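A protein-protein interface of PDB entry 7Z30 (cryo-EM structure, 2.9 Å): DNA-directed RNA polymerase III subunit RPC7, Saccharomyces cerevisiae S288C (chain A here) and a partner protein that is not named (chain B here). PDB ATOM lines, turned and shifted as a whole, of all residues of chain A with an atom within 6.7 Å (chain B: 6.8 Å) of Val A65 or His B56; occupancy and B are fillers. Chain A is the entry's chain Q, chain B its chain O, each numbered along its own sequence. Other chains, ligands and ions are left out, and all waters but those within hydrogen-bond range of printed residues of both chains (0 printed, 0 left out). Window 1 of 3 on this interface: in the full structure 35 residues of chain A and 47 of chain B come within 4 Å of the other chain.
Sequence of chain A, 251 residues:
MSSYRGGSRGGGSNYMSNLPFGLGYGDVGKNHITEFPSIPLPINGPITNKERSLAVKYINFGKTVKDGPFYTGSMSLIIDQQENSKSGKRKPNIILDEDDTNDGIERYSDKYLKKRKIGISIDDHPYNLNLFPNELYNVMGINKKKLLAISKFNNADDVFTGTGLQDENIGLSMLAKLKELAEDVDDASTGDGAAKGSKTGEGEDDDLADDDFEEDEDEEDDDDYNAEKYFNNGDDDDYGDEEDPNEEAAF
Of chain B, only His B56 and Ser B165 come within 4 Å of Val A65.
His B56 touches just one residue of chain A: Val A65.
Of the printed residues of chain A, Leu B130 touches Phe A61.
Of the printed residues of chain A, Ile B164 touches Phe A61.
The nearest printed residue of chain B that does not touch Val A65 is Leu B57 (4.9 Å).
The nearest residue of chain A that does not touch His B56 is Phe A61 (4.1 Å).
The nearest printed residue of chain A that does not touch Ile B164 is Thr A64 (5.7 Å).
NE2 of Gln B161 touches O of Asn A60, at 3.9 Å.
Ser B133 touches Phe A61.
Ile B164 touches Phe A61.
CG2 of Thr A64 touches NE2 of Gln B161, 3.4 Å away.
CG2 of Thr A64 touches OG of Ser B165, at 3.8 Å.
Val A65 touches His B56.
O of Ser B165 touches CG2 of Val A65, at 3.8 Å.
Leu B57 touches Phe A70.
Ser B165 touches Phe A70.
O of Tyr A71 touches CA of Gly B58 (3.8 Å).
Of the 19 printed residues of chain B, 10 touch a printed residue of chain A.
Hydrophobic or aromatic side chains of chain B that line the printed part of chain A: Leu B101, Leu B130, Ile B164 and Leu B166.
Of the 12 printed residues of chain A, 6 touch a printed residue of chain B.
Printed residues of chain A that touch a printed residue of chain B: Asn A60, Phe A61, Thr A64, Val A65, Phe A70 and Tyr A71.
Among the printed residues, 14 pairs touch across the chains.
Among the printed residues, no Asp or Glu carboxylate lies within 4 Å of a Lys or Arg side-chain nitrogen of the other chain.
The backbone carbonyl oxygen (O) of Tyr A71 lies close to the backbone carbonyl oxygen (O) of Leu B57 (2.7 Å).
The backbone carbonyl oxygen (O) of Val B53 sits at hydrogen-bond distance from the backbone NH (N) of Gly B58, 3.1 Å away.
OG of Ser B133 lies within hydrogen-bond range of O of Leu B130, 2.8 Å away.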
ATOM      1  N   ASN A  60      17.140 -15.022   1.325  1.00  0.00           N
ATOM      2  CA  ASN A  60      17.308 -16.476   1.384  1.00  0.00           C
ATOM      3  C   ASN A  60      18.603 -16.851   2.099  1.00  0.00           C
ATOM      4  O   ASN A  60      18.626 -17.788   2.910  1.00  0.00           O
ATOM      5  CB  ASN A  60      17.275 -17.116  -0.007  1.00  0.00           C
ATOM      6  CG  ASN A  60      16.158 -16.589  -0.879  1.00  0.00           C
ATOM      7  OD1 ASN A  60      16.389 -16.165  -2.010  1.00  0.00           O
ATOM      8  ND2 ASN A  60      14.938 -16.610  -0.357  1.00  0.00           N
ATOM      9  N   PHE A  61      19.691 -16.144   1.803  1.00  0.00           N
ATOM     10  CA  PHE A  61      20.910 -16.331   2.572  1.00  0.00           C
ATOM     11  C   PHE A  61      20.724 -15.766   3.979  1.00  0.00           C
ATOM     12  O   PHE A  61      19.843 -14.941   4.235  1.00  0.00           O
ATOM     13  CB  PHE A  61      22.104 -15.663   1.889  1.00  0.00           C
ATOM     14  CG  PHE A  61      23.404 -15.879   2.609  1.00  0.00           C
ATOM     15  CD1 PHE A  61      23.925 -17.155   2.752  1.00  0.00           C
ATOM     16  CD2 PHE A  61      24.088 -14.817   3.172  1.00  0.00           C
ATOM     17  CE1 PHE A  61      25.113 -17.362   3.423  1.00  0.00           C
ATOM     18  CE2 PHE A  61      25.279 -15.019   3.843  1.00  0.00           C
ATOM     19  CZ  PHE A  61      25.791 -16.293   3.969  1.00  0.00           C
ATOM     20  N   GLY A  62      21.552 -16.234   4.901  1.00  0.00           N
ATOM     21  CA  GLY A  62      21.352 -15.865   6.299  1.00  0.00           C
ATOM     22  C   GLY A  62      20.199 -16.622   6.905  1.00  0.00           C
ATOM     23  O   GLY A  62      20.354 -17.255   7.953  1.00  0.00           O
ATOM     24  N   LYS A  63      19.034 -16.590   6.254  1.00  0.00           N
ATOM     25  CA  LYS A  63      17.949 -17.482   6.640  1.00  0.00           C
ATOM     26  C   LYS A  63      18.370 -18.937   6.497  1.00  0.00           C
ATOM     27  O   LYS A  63      18.031 -19.774   7.340  1.00  0.00           O
ATOM     28  CB  LYS A  63      16.710 -17.200   5.792  1.00  0.00           C
ATOM     29  CG  LYS A  63      15.507 -18.063   6.133  1.00  0.00           C
ATOM     30  CD  LYS A  63      14.523 -18.104   4.974  1.00  0.00           C
ATOM     31  CE  LYS A  63      14.011 -16.713   4.632  1.00  0.00           C
ATOM     32  NZ  LYS A  63      12.769 -16.770   3.812  1.00  0.00           N
ATOM     33  N   THR A  64      19.108 -19.259   5.430  1.00  0.00           N
ATOM     34  CA  THR A  64      19.592 -20.628   5.267  1.00  0.00           C
ATOM     35  C   THR A  64      20.552 -21.022   6.389  1.00  0.00           C
ATOM     36  O   THR A  64      20.460 -22.130   6.933  1.00  0.00           O
ATOM     37  CB  THR A  64      20.238 -20.798   3.886  1.00  0.00           C
ATOM     38  OG1 THR A  64      20.558 -22.179   3.668  1.00  0.00           O
ATOM     39  CG2 THR A  64      21.495 -19.942   3.730  1.00  0.00           C
ATOM     40  N   VAL A  65      21.455 -20.120   6.778  1.00  0.00           N
ATOM     41  CA  VAL A  65      22.433 -20.459   7.806  1.00  0.00           C
ATOM     42  C   VAL A  65      21.798 -20.451   9.193  1.00  0.00           C
ATOM     43  O   VAL A  65      22.317 -21.084  10.120  1.00  0.00           O
ATOM     44  CB  VAL A  65      23.643 -19.511   7.727  1.00  0.00           C
ATOM     45  CG1 VAL A  65      23.373 -18.221   8.483  1.00  0.00           C
ATOM     46  CG2 VAL A  65      24.891 -20.196   8.263  1.00  0.00           C
ATOM     47  N   LYS A  66      20.673 -19.754   9.361  1.00  0.00           N
ATOM     48  CA  LYS A  66      19.993 -19.743  10.649  1.00  0.00           C
ATOM     49  C   LYS A  66      19.054 -20.933  10.803  1.00  0.00           C
ATOM     50  O   LYS A  66      18.905 -21.458  11.912  1.00  0.00           O
ATOM     51  CB  LYS A  66      19.228 -18.432  10.823  1.00  0.00           C
ATOM     52  CG  LYS A  66      19.228 -17.900  12.243  1.00  0.00           C
ATOM     53  CD  LYS A  66      18.059 -16.968  12.483  1.00  0.00           C
ATOM     54  CE  LYS A  66      18.316 -16.076  13.685  1.00  0.00           C
ATOM     55  NZ  LYS A  66      17.280 -15.017  13.819  1.00  0.00           N
ATOM     56  N   ASP A  67      18.415 -21.368   9.715  1.00  0.00           N
ATOM     57  CA  ASP A  67      17.649 -22.607   9.740  1.00  0.00           C
ATOM     58  C   ASP A  67      18.543 -23.838   9.695  1.00  0.00           C
ATOM     59  O   ASP A  67      18.072 -24.941   9.990  1.00  0.00           O
ATOM     60  CB  ASP A  67      16.654 -22.640   8.577  1.00  0.00           C
ATOM     61  CG  ASP A  67      15.508 -21.664   8.763  1.00  0.00           C
ATOM     62  OD1 ASP A  67      15.061 -21.483   9.915  1.00  0.00           O
ATOM     63  OD2 ASP A  67      15.050 -21.078   7.759  1.00  0.00           O
ATOM     64  N   GLY A  68      19.817 -23.674   9.334  1.00  0.00           N
ATOM     65  CA  GLY A  68      20.765 -24.754   9.442  1.00  0.00           C
ATOM     66  C   GLY A  68      21.232 -24.951  10.867  1.00  0.00           C
ATOM     67  O   GLY A  68      20.681 -24.396  11.827  1.00  0.00           O
ATOM     68  N   PRO A  69      22.275 -25.765  11.024  1.00  0.00           N
ATOM     69  CA  PRO A  69      22.830 -26.025  12.355  1.00  0.00           C
ATOM     70  C   PRO A  69      23.755 -24.939  12.883  1.00  0.00           C
ATOM     71  O   PRO A  69      24.153 -25.011  14.049  1.00  0.00           O
ATOM     72  CB  PRO A  69      23.604 -27.334  12.138  1.00  0.00           C
ATOM     73  CG  PRO A  69      24.071 -27.243  10.727  1.00  0.00           C
ATOM     74  CD  PRO A  69      22.996 -26.499   9.967  1.00  0.00           C
ATOM     75  N   PHE A  70      24.102 -23.939  12.077  1.00  0.00           N
ATOM     76  CA  PHE A  70      25.080 -22.931  12.483  1.00  0.00           C
ATOM     77  C   PHE A  70      24.370 -21.704  13.051  1.00  0.00           C
ATOM     78  O   PHE A  70      24.350 -20.622  12.460  1.00  0.00           O
ATOM     79  CB  PHE A  70      25.976 -22.559  11.305  1.00  0.00           C
ATOM     80  CG  PHE A  70      26.677 -23.729  10.682  1.00  0.00           C
ATOM     81  CD1 PHE A  70      27.063 -24.812  11.452  1.00  0.00           C
ATOM     82  CD2 PHE A  70      26.956 -23.744   9.326  1.00  0.00           C
ATOM     83  CE1 PHE A  70      27.705 -25.887  10.881  1.00  0.00           C
ATOM     84  CE2 PHE A  70      27.602 -24.818   8.749  1.00  0.00           C
ATOM     85  CZ  PHE A  70      27.977 -25.893   9.529  1.00  0.00           C
ATOM     86  N   TYR A  71      23.771 -21.888  14.228  1.00  0.00           N
ATOM     87  CA  TYR A  71      23.245 -20.771  15.001  1.00  0.00           C
ATOM     88  C   TYR A  71      24.182 -20.380  16.136  1.00  0.00           C
ATOM     89  O   TYR A  71      24.693 -19.256  16.153  1.00  0.00           O
ATOM     90  CB  TYR A  71      21.855 -21.108  15.557  1.00  0.00           C
ATOM     91  CG  TYR A  71      21.176 -19.939  16.241  1.00  0.00           C
ATOM     92  CD1 TYR A  71      21.383 -18.639  15.802  1.00  0.00           C
ATOM     93  CD2 TYR A  71      20.325 -20.136  17.319  1.00  0.00           C
ATOM     94  CE1 TYR A  71      20.769 -17.567  16.421  1.00  0.00           C
ATOM     95  CE2 TYR A  71      19.704 -19.069  17.945  1.00  0.00           C
ATOM     96  CZ  TYR A  71      19.930 -17.787  17.490  1.00  0.00           C
ATOM     97  OH  TYR A  71      19.317 -16.721  18.106  1.00  0.00           O
ATOM     98  N   GLU B  51      28.269  -6.626  13.513  1.00  0.00           N
ATOM     99  CA  GLU B  51      26.899  -6.612  13.013  1.00  0.00           C
ATOM    100  C   GLU B  51      26.656  -7.744  12.022  1.00  0.00           C
ATOM    101  O   GLU B  51      25.581  -8.356  12.021  1.00  0.00           O
ATOM    102  CB  GLU B  51      26.598  -5.260  12.369  1.00  0.00           C
ATOM    103  CG  GLU B  51      25.149  -4.828  12.479  1.00  0.00           C
ATOM    104  CD  GLU B  51      24.560  -5.112  13.844  1.00  0.00           C
ATOM    105  OE1 GLU B  51      24.998  -4.477  14.826  1.00  0.00           O
ATOM    106  OE2 GLU B  51      23.658  -5.969  13.935  1.00  0.00           O
ATOM    107  N   LEU B  52      27.641  -8.031  11.167  1.00  0.00           N
ATOM    108  CA  LEU B  52      27.491  -9.114  10.199  1.00  0.00           C
ATOM    109  C   LEU B  52      27.304 -10.456  10.897  1.00  0.00           C
ATOM    110  O   LEU B  52      26.405 -11.233  10.549  1.00  0.00           O
ATOM    111  CB  LEU B  52      28.707  -9.159   9.277  1.00  0.00           C
ATOM    112  CG  LEU B  52      28.753  -8.149   8.133  1.00  0.00           C
ATOM    113  CD1 LEU B  52      29.791  -8.582   7.125  1.00  0.00           C
ATOM    114  CD2 LEU B  52      27.388  -8.018   7.476  1.00  0.00           C
ATOM    115  N   VAL B  53      28.150 -10.745  11.886  1.00  0.00           N
ATOM    116  CA  VAL B  53      28.032 -12.016  12.596  1.00  0.00           C
ATOM    117  C   VAL B  53      26.748 -12.054  13.414  1.00  0.00           C
ATOM    118  O   VAL B  53      26.104 -13.103  13.529  1.00  0.00           O
ATOM    119  CB  VAL B  53      29.278 -12.271  13.460  1.00  0.00           C
ATOM    120  CG1 VAL B  53      29.229 -13.671  14.043  1.00  0.00           C
ATOM    121  CG2 VAL B  53      30.524 -12.109  12.617  1.00  0.00           C
ATOM    122  N   LYS B  54      26.349 -10.911  13.983  1.00  0.00           N
ATOM    123  CA  LYS B  54      25.050 -10.816  14.643  1.00  0.00           C
ATOM    124  C   LYS B  54      23.921 -11.222  13.709  1.00  0.00           C
ATOM    125  O   LYS B  54      23.043 -12.008  14.084  1.00  0.00           O
ATOM    126  CB  LYS B  54      24.825  -9.382  15.139  1.00  0.00           C
ATOM    127  CG  LYS B  54      25.233  -9.062  16.582  1.00  0.00           C
ATOM    128  CD  LYS B  54      24.697 -10.022  17.663  1.00  0.00           C
ATOM    129  CE  LYS B  54      23.287 -10.560  17.386  1.00  0.00           C
ATOM    130  NZ  LYS B  54      22.250  -9.538  17.693  1.00  0.00           N
ATOM    131  N   ALA B  55      23.928 -10.692  12.488  1.00  0.00           N
ATOM    132  CA  ALA B  55      22.857 -10.989  11.545  1.00  0.00           C
ATOM    133  C   ALA B  55      22.882 -12.448  11.109  1.00  0.00           C
ATOM    134  O   ALA B  55      21.828 -13.084  10.985  1.00  0.00           O
ATOM    135  CB  ALA B  55      22.960 -10.065  10.332  1.00  0.00           C
ATOM    136  N   HIS B  56      24.073 -12.999  10.872  1.00  0.00           N
ATOM    137  CA  HIS B  56      24.150 -14.291  10.197  1.00  0.00           C
ATOM    138  C   HIS B  56      24.228 -15.456  11.180  1.00  0.00           C
ATOM    139  O   HIS B  56      23.389 -16.363  11.146  1.00  0.00           O
ATOM    140  CB  HIS B  56      25.334 -14.292   9.231  1.00  0.00           C
ATOM    141  CG  HIS B  56      25.241 -13.232   8.178  1.00  0.00           C
ATOM    142  ND1 HIS B  56      26.278 -12.930   7.323  1.00  0.00           N
ATOM    143  CD2 HIS B  56      24.223 -12.405   7.839  1.00  0.00           C
ATOM    144  CE1 HIS B  56      25.907 -11.958   6.509  1.00  0.00           C
ATOM    145  NE2 HIS B  56      24.664 -11.622   6.800  1.00  0.00           N
ATOM    146  N   LEU B  57      25.222 -15.458  12.068  1.00  0.00           N
ATOM    147  CA  LEU B  57      25.428 -16.638  12.905  1.00  0.00           C
ATOM    148  C   LEU B  57      24.646 -16.560  14.214  1.00  0.00           C
ATOM    149  O   LEU B  57      23.752 -17.375  14.453  1.00  0.00           O
ATOM    150  CB  LEU B  57      26.924 -16.835  13.174  1.00  0.00           C
ATOM    151  CG  LEU B  57      27.655 -17.656  12.108  1.00  0.00           C
ATOM    152  CD1 LEU B  57      28.329 -16.752  11.089  1.00  0.00           C
ATOM    153  CD2 LEU B  57      28.660 -18.600  12.743  1.00  0.00           C
ATOM    154  N   GLY B  58      24.946 -15.576  15.050  1.00  0.00           N
ATOM    155  CA  GLY B  58      24.288 -15.472  16.336  1.00  0.00           C
ATOM    156  C   GLY B  58      25.027 -14.507  17.235  1.00  0.00           C
ATOM    157  O   GLY B  58      26.114 -14.023  16.908  1.00  0.00           O
ATOM    158  N   LEU B 101      32.933 -21.661   9.746  1.00  0.00           N
ATOM    159  CA  LEU B 101      32.499 -20.575   8.876  1.00  0.00           C
ATOM    160  C   LEU B 101      33.659 -19.781   8.283  1.00  0.00           C
ATOM    161  O   LEU B 101      33.409 -18.767   7.621  1.00  0.00           O
ATOM    162  CB  LEU B 101      31.560 -19.633   9.633  1.00  0.00           C
ATOM    163  CG  LEU B 101      30.067 -19.857   9.386  1.00  0.00           C
ATOM    164  CD1 LEU B 101      29.770 -19.820   7.894  1.00  0.00           C
ATOM    165  CD2 LEU B 101      29.601 -21.169   9.994  1.00  0.00           C
ATOM    166  N   ILE B 127      35.026 -13.467   6.243  1.00  0.00           N
ATOM    167  CA  ILE B 127      33.725 -12.851   6.483  1.00  0.00           C
ATOM    168  C   ILE B 127      33.143 -12.186   5.245  1.00  0.00           C
ATOM    169  O   ILE B 127      31.933 -11.917   5.196  1.00  0.00           O
ATOM    170  CB  ILE B 127      33.832 -11.840   7.640  1.00  0.00           C
ATOM    171  CG1 ILE B 127      34.621 -10.614   7.195  1.00  0.00           C
ATOM    172  CG2 ILE B 127      34.479 -12.488   8.855  1.00  0.00           C
ATOM    173  CD1 ILE B 127      34.930  -9.675   8.307  1.00  0.00           C
ATOM    174  N   LEU B 130      30.228 -14.505   3.474  1.00  0.00           N
ATOM    175  CA  LEU B 130      28.821 -14.289   3.907  1.00  0.00           C
ATOM    176  C   LEU B 130      28.375 -12.885   3.484  1.00  0.00           C
ATOM    177  O   LEU B 130      27.206 -12.729   3.089  1.00  0.00           O
ATOM    178  CB  LEU B 130      28.727 -14.467   5.426  1.00  0.00           C
ATOM    179  CG  LEU B 130      30.027 -14.258   6.199  1.00  0.00           C
ATOM    180  CD1 LEU B 130      29.807 -13.334   7.387  1.00  0.00           C
ATOM    181  CD2 LEU B 130      30.607 -15.586   6.658  1.00  0.00           C
ATOM    182  N   LEU B 131      29.278 -11.905   3.568  1.00  0.00           N
ATOM    183  CA  LEU B 131      28.940 -10.512   3.176  1.00  0.00           C
ATOM    184  C   LEU B 131      28.703 -10.455   1.662  1.00  0.00           C
ATOM    185  O   LEU B 131      27.588 -10.072   1.258  1.00  0.00           O
ATOM    186  CB  LEU B 131      30.080  -9.582   3.607  1.00  0.00           C
ATOM    187  CG  LEU B 131      30.249  -8.311   2.778  1.00  0.00           C
ATOM    188  CD1 LEU B 131      30.082  -7.072   3.644  1.00  0.00           C
ATOM    189  CD2 LEU B 131      31.605  -8.302   2.096  1.00  0.00           C
ATOM    190  N   SER B 133      27.987 -12.623  -0.313  1.00  0.00           N
ATOM    191  CA  SER B 133      27.275 -13.818  -0.757  1.00  0.00           C
ATOM    192  C   SER B 133      26.383 -13.530  -1.958  1.00  0.00           C
ATOM    193  O   SER B 133      26.425 -14.251  -2.963  1.00  0.00           O
ATOM    194  CB  SER B 133      26.451 -14.380   0.399  1.00  0.00           C
ATOM    195  OG  SER B 133      25.604 -13.378   0.933  1.00  0.00           O
ATOM    196  N   GLN B 161      25.198 -21.619  -3.197  1.00  0.00           N
ATOM    197  CA  GLN B 161      24.579 -21.222  -1.936  1.00  0.00           C
ATOM    198  C   GLN B 161      24.880 -22.224  -0.828  1.00  0.00           C
ATOM    199  O   GLN B 161      25.202 -21.841   0.300  1.00  0.00           O
ATOM    200  CB  GLN B 161      23.069 -21.063  -2.120  1.00  0.00           C
ATOM    201  CG  GLN B 161      22.445 -20.040  -1.194  1.00  0.00           C
ATOM    202  CD  GLN B 161      21.608 -20.690  -0.114  1.00  0.00           C
ATOM    203  OE1 GLN B 161      21.840 -21.841   0.249  1.00  0.00           O
ATOM    204  NE2 GLN B 161      20.657 -19.944   0.433  1.00  0.00           N
ATOM    205  N   ILE B 164      28.535 -21.693   0.222  1.00  0.00           N
ATOM    206  CA  ILE B 164      28.900 -20.524   1.019  1.00  0.00           C
ATOM    207  C   ILE B 164      28.213 -20.591   2.383  1.00  0.00           C
ATOM    208  O   ILE B 164      28.702 -20.008   3.356  1.00  0.00           O
ATOM    209  CB  ILE B 164      28.643 -19.174   0.295  1.00  0.00           C
ATOM    210  CG1 ILE B 164      27.275 -18.992  -0.372  1.00  0.00           C
ATOM    211  CG2 ILE B 164      29.701 -18.918  -0.763  1.00  0.00           C
ATOM    212  CD1 ILE B 164      26.088 -19.083   0.533  1.00  0.00           C
ATOM    213  N   SER B 165      27.081 -21.297   2.482  1.00  0.00           N
ATOM    214  CA  SER B 165      26.389 -21.396   3.761  1.00  0.00           C
ATOM    215  C   SER B 165      26.988 -22.477   4.650  1.00  0.00           C
ATOM    216  O   SER B 165      26.880 -22.394   5.878  1.00  0.00           O
ATOM    217  CB  SER B 165      24.902 -21.658   3.526  1.00  0.00           C
ATOM    218  OG  SER B 165      24.307 -22.239   4.672  1.00  0.00           O
ATOM    219  N   LEU B 166      27.624 -23.491   4.061  1.00  0.00           N
ATOM    220  CA  LEU B 166      28.203 -24.583   4.828  1.00  0.00           C
ATOM    221  C   LEU B 166      29.707 -24.464   5.018  1.00  0.00           C
ATOM    222  O   LEU B 166      30.242 -25.075   5.947  1.00  0.00           O
ATOM    223  CB  LEU B 166      27.888 -25.930   4.163  1.00  0.00           C
ATOM    224  CG  LEU B 166      26.555 -26.606   4.499  1.00  0.00           C
ATOM    225  CD1 LEU B 166      26.346 -26.681   6.005  1.00  0.00           C
ATOM    226  CD2 LEU B 166      25.389 -25.897   3.834  1.00  0.00           C
ATOM    227  N   LEU B 589      23.434  -2.498   8.260  1.00  0.00           N
ATOM    228  CA  LEU B 589      23.129  -3.775   8.908  1.00  0.00           C
ATOM    229  C   LEU B 589      22.502  -3.573  10.282  1.00  0.00           C
ATOM    230  O   LEU B 589      21.643  -4.358  10.693  1.00  0.00           O
ATOM    231  CB  LEU B 589      24.353  -4.691   9.008  1.00  0.00           C
ATOM    232  CG  LEU B 589      25.148  -5.125   7.771  1.00  0.00           C
ATOM    233  CD1 LEU B 589      24.208  -5.396   6.605  1.00  0.00           C
ATOM    234  CD2 LEU B 589      26.278  -4.205   7.380  1.00  0.00           C
ATOM    235  N   GLU B 593      18.910  -5.137  11.139  1.00  0.00           N
ATOM    236  CA  GLU B 593      18.798  -6.063  12.259  1.00  0.00           C
ATOM    237  C   GLU B 593      17.899  -5.514  13.358  1.00  0.00           C
ATOM    238  O   GLU B 593      17.223  -6.286  14.038  1.00  0.00           O
ATOM    239  CB  GLU B 593      20.182  -6.399  12.819  1.00  0.00           C
ATOM    240  CG  GLU B 593      20.243  -7.561  13.837  1.00  0.00           C
ATOM    241  CD  GLU B 593      19.363  -8.776  13.518  1.00  0.00           C
ATOM    242  OE1 GLU B 593      19.190  -9.616  14.425  1.00  0.00           O
ATOM    243  OE2 GLU B 593      18.905  -8.951  12.369  1.00  0.00           O
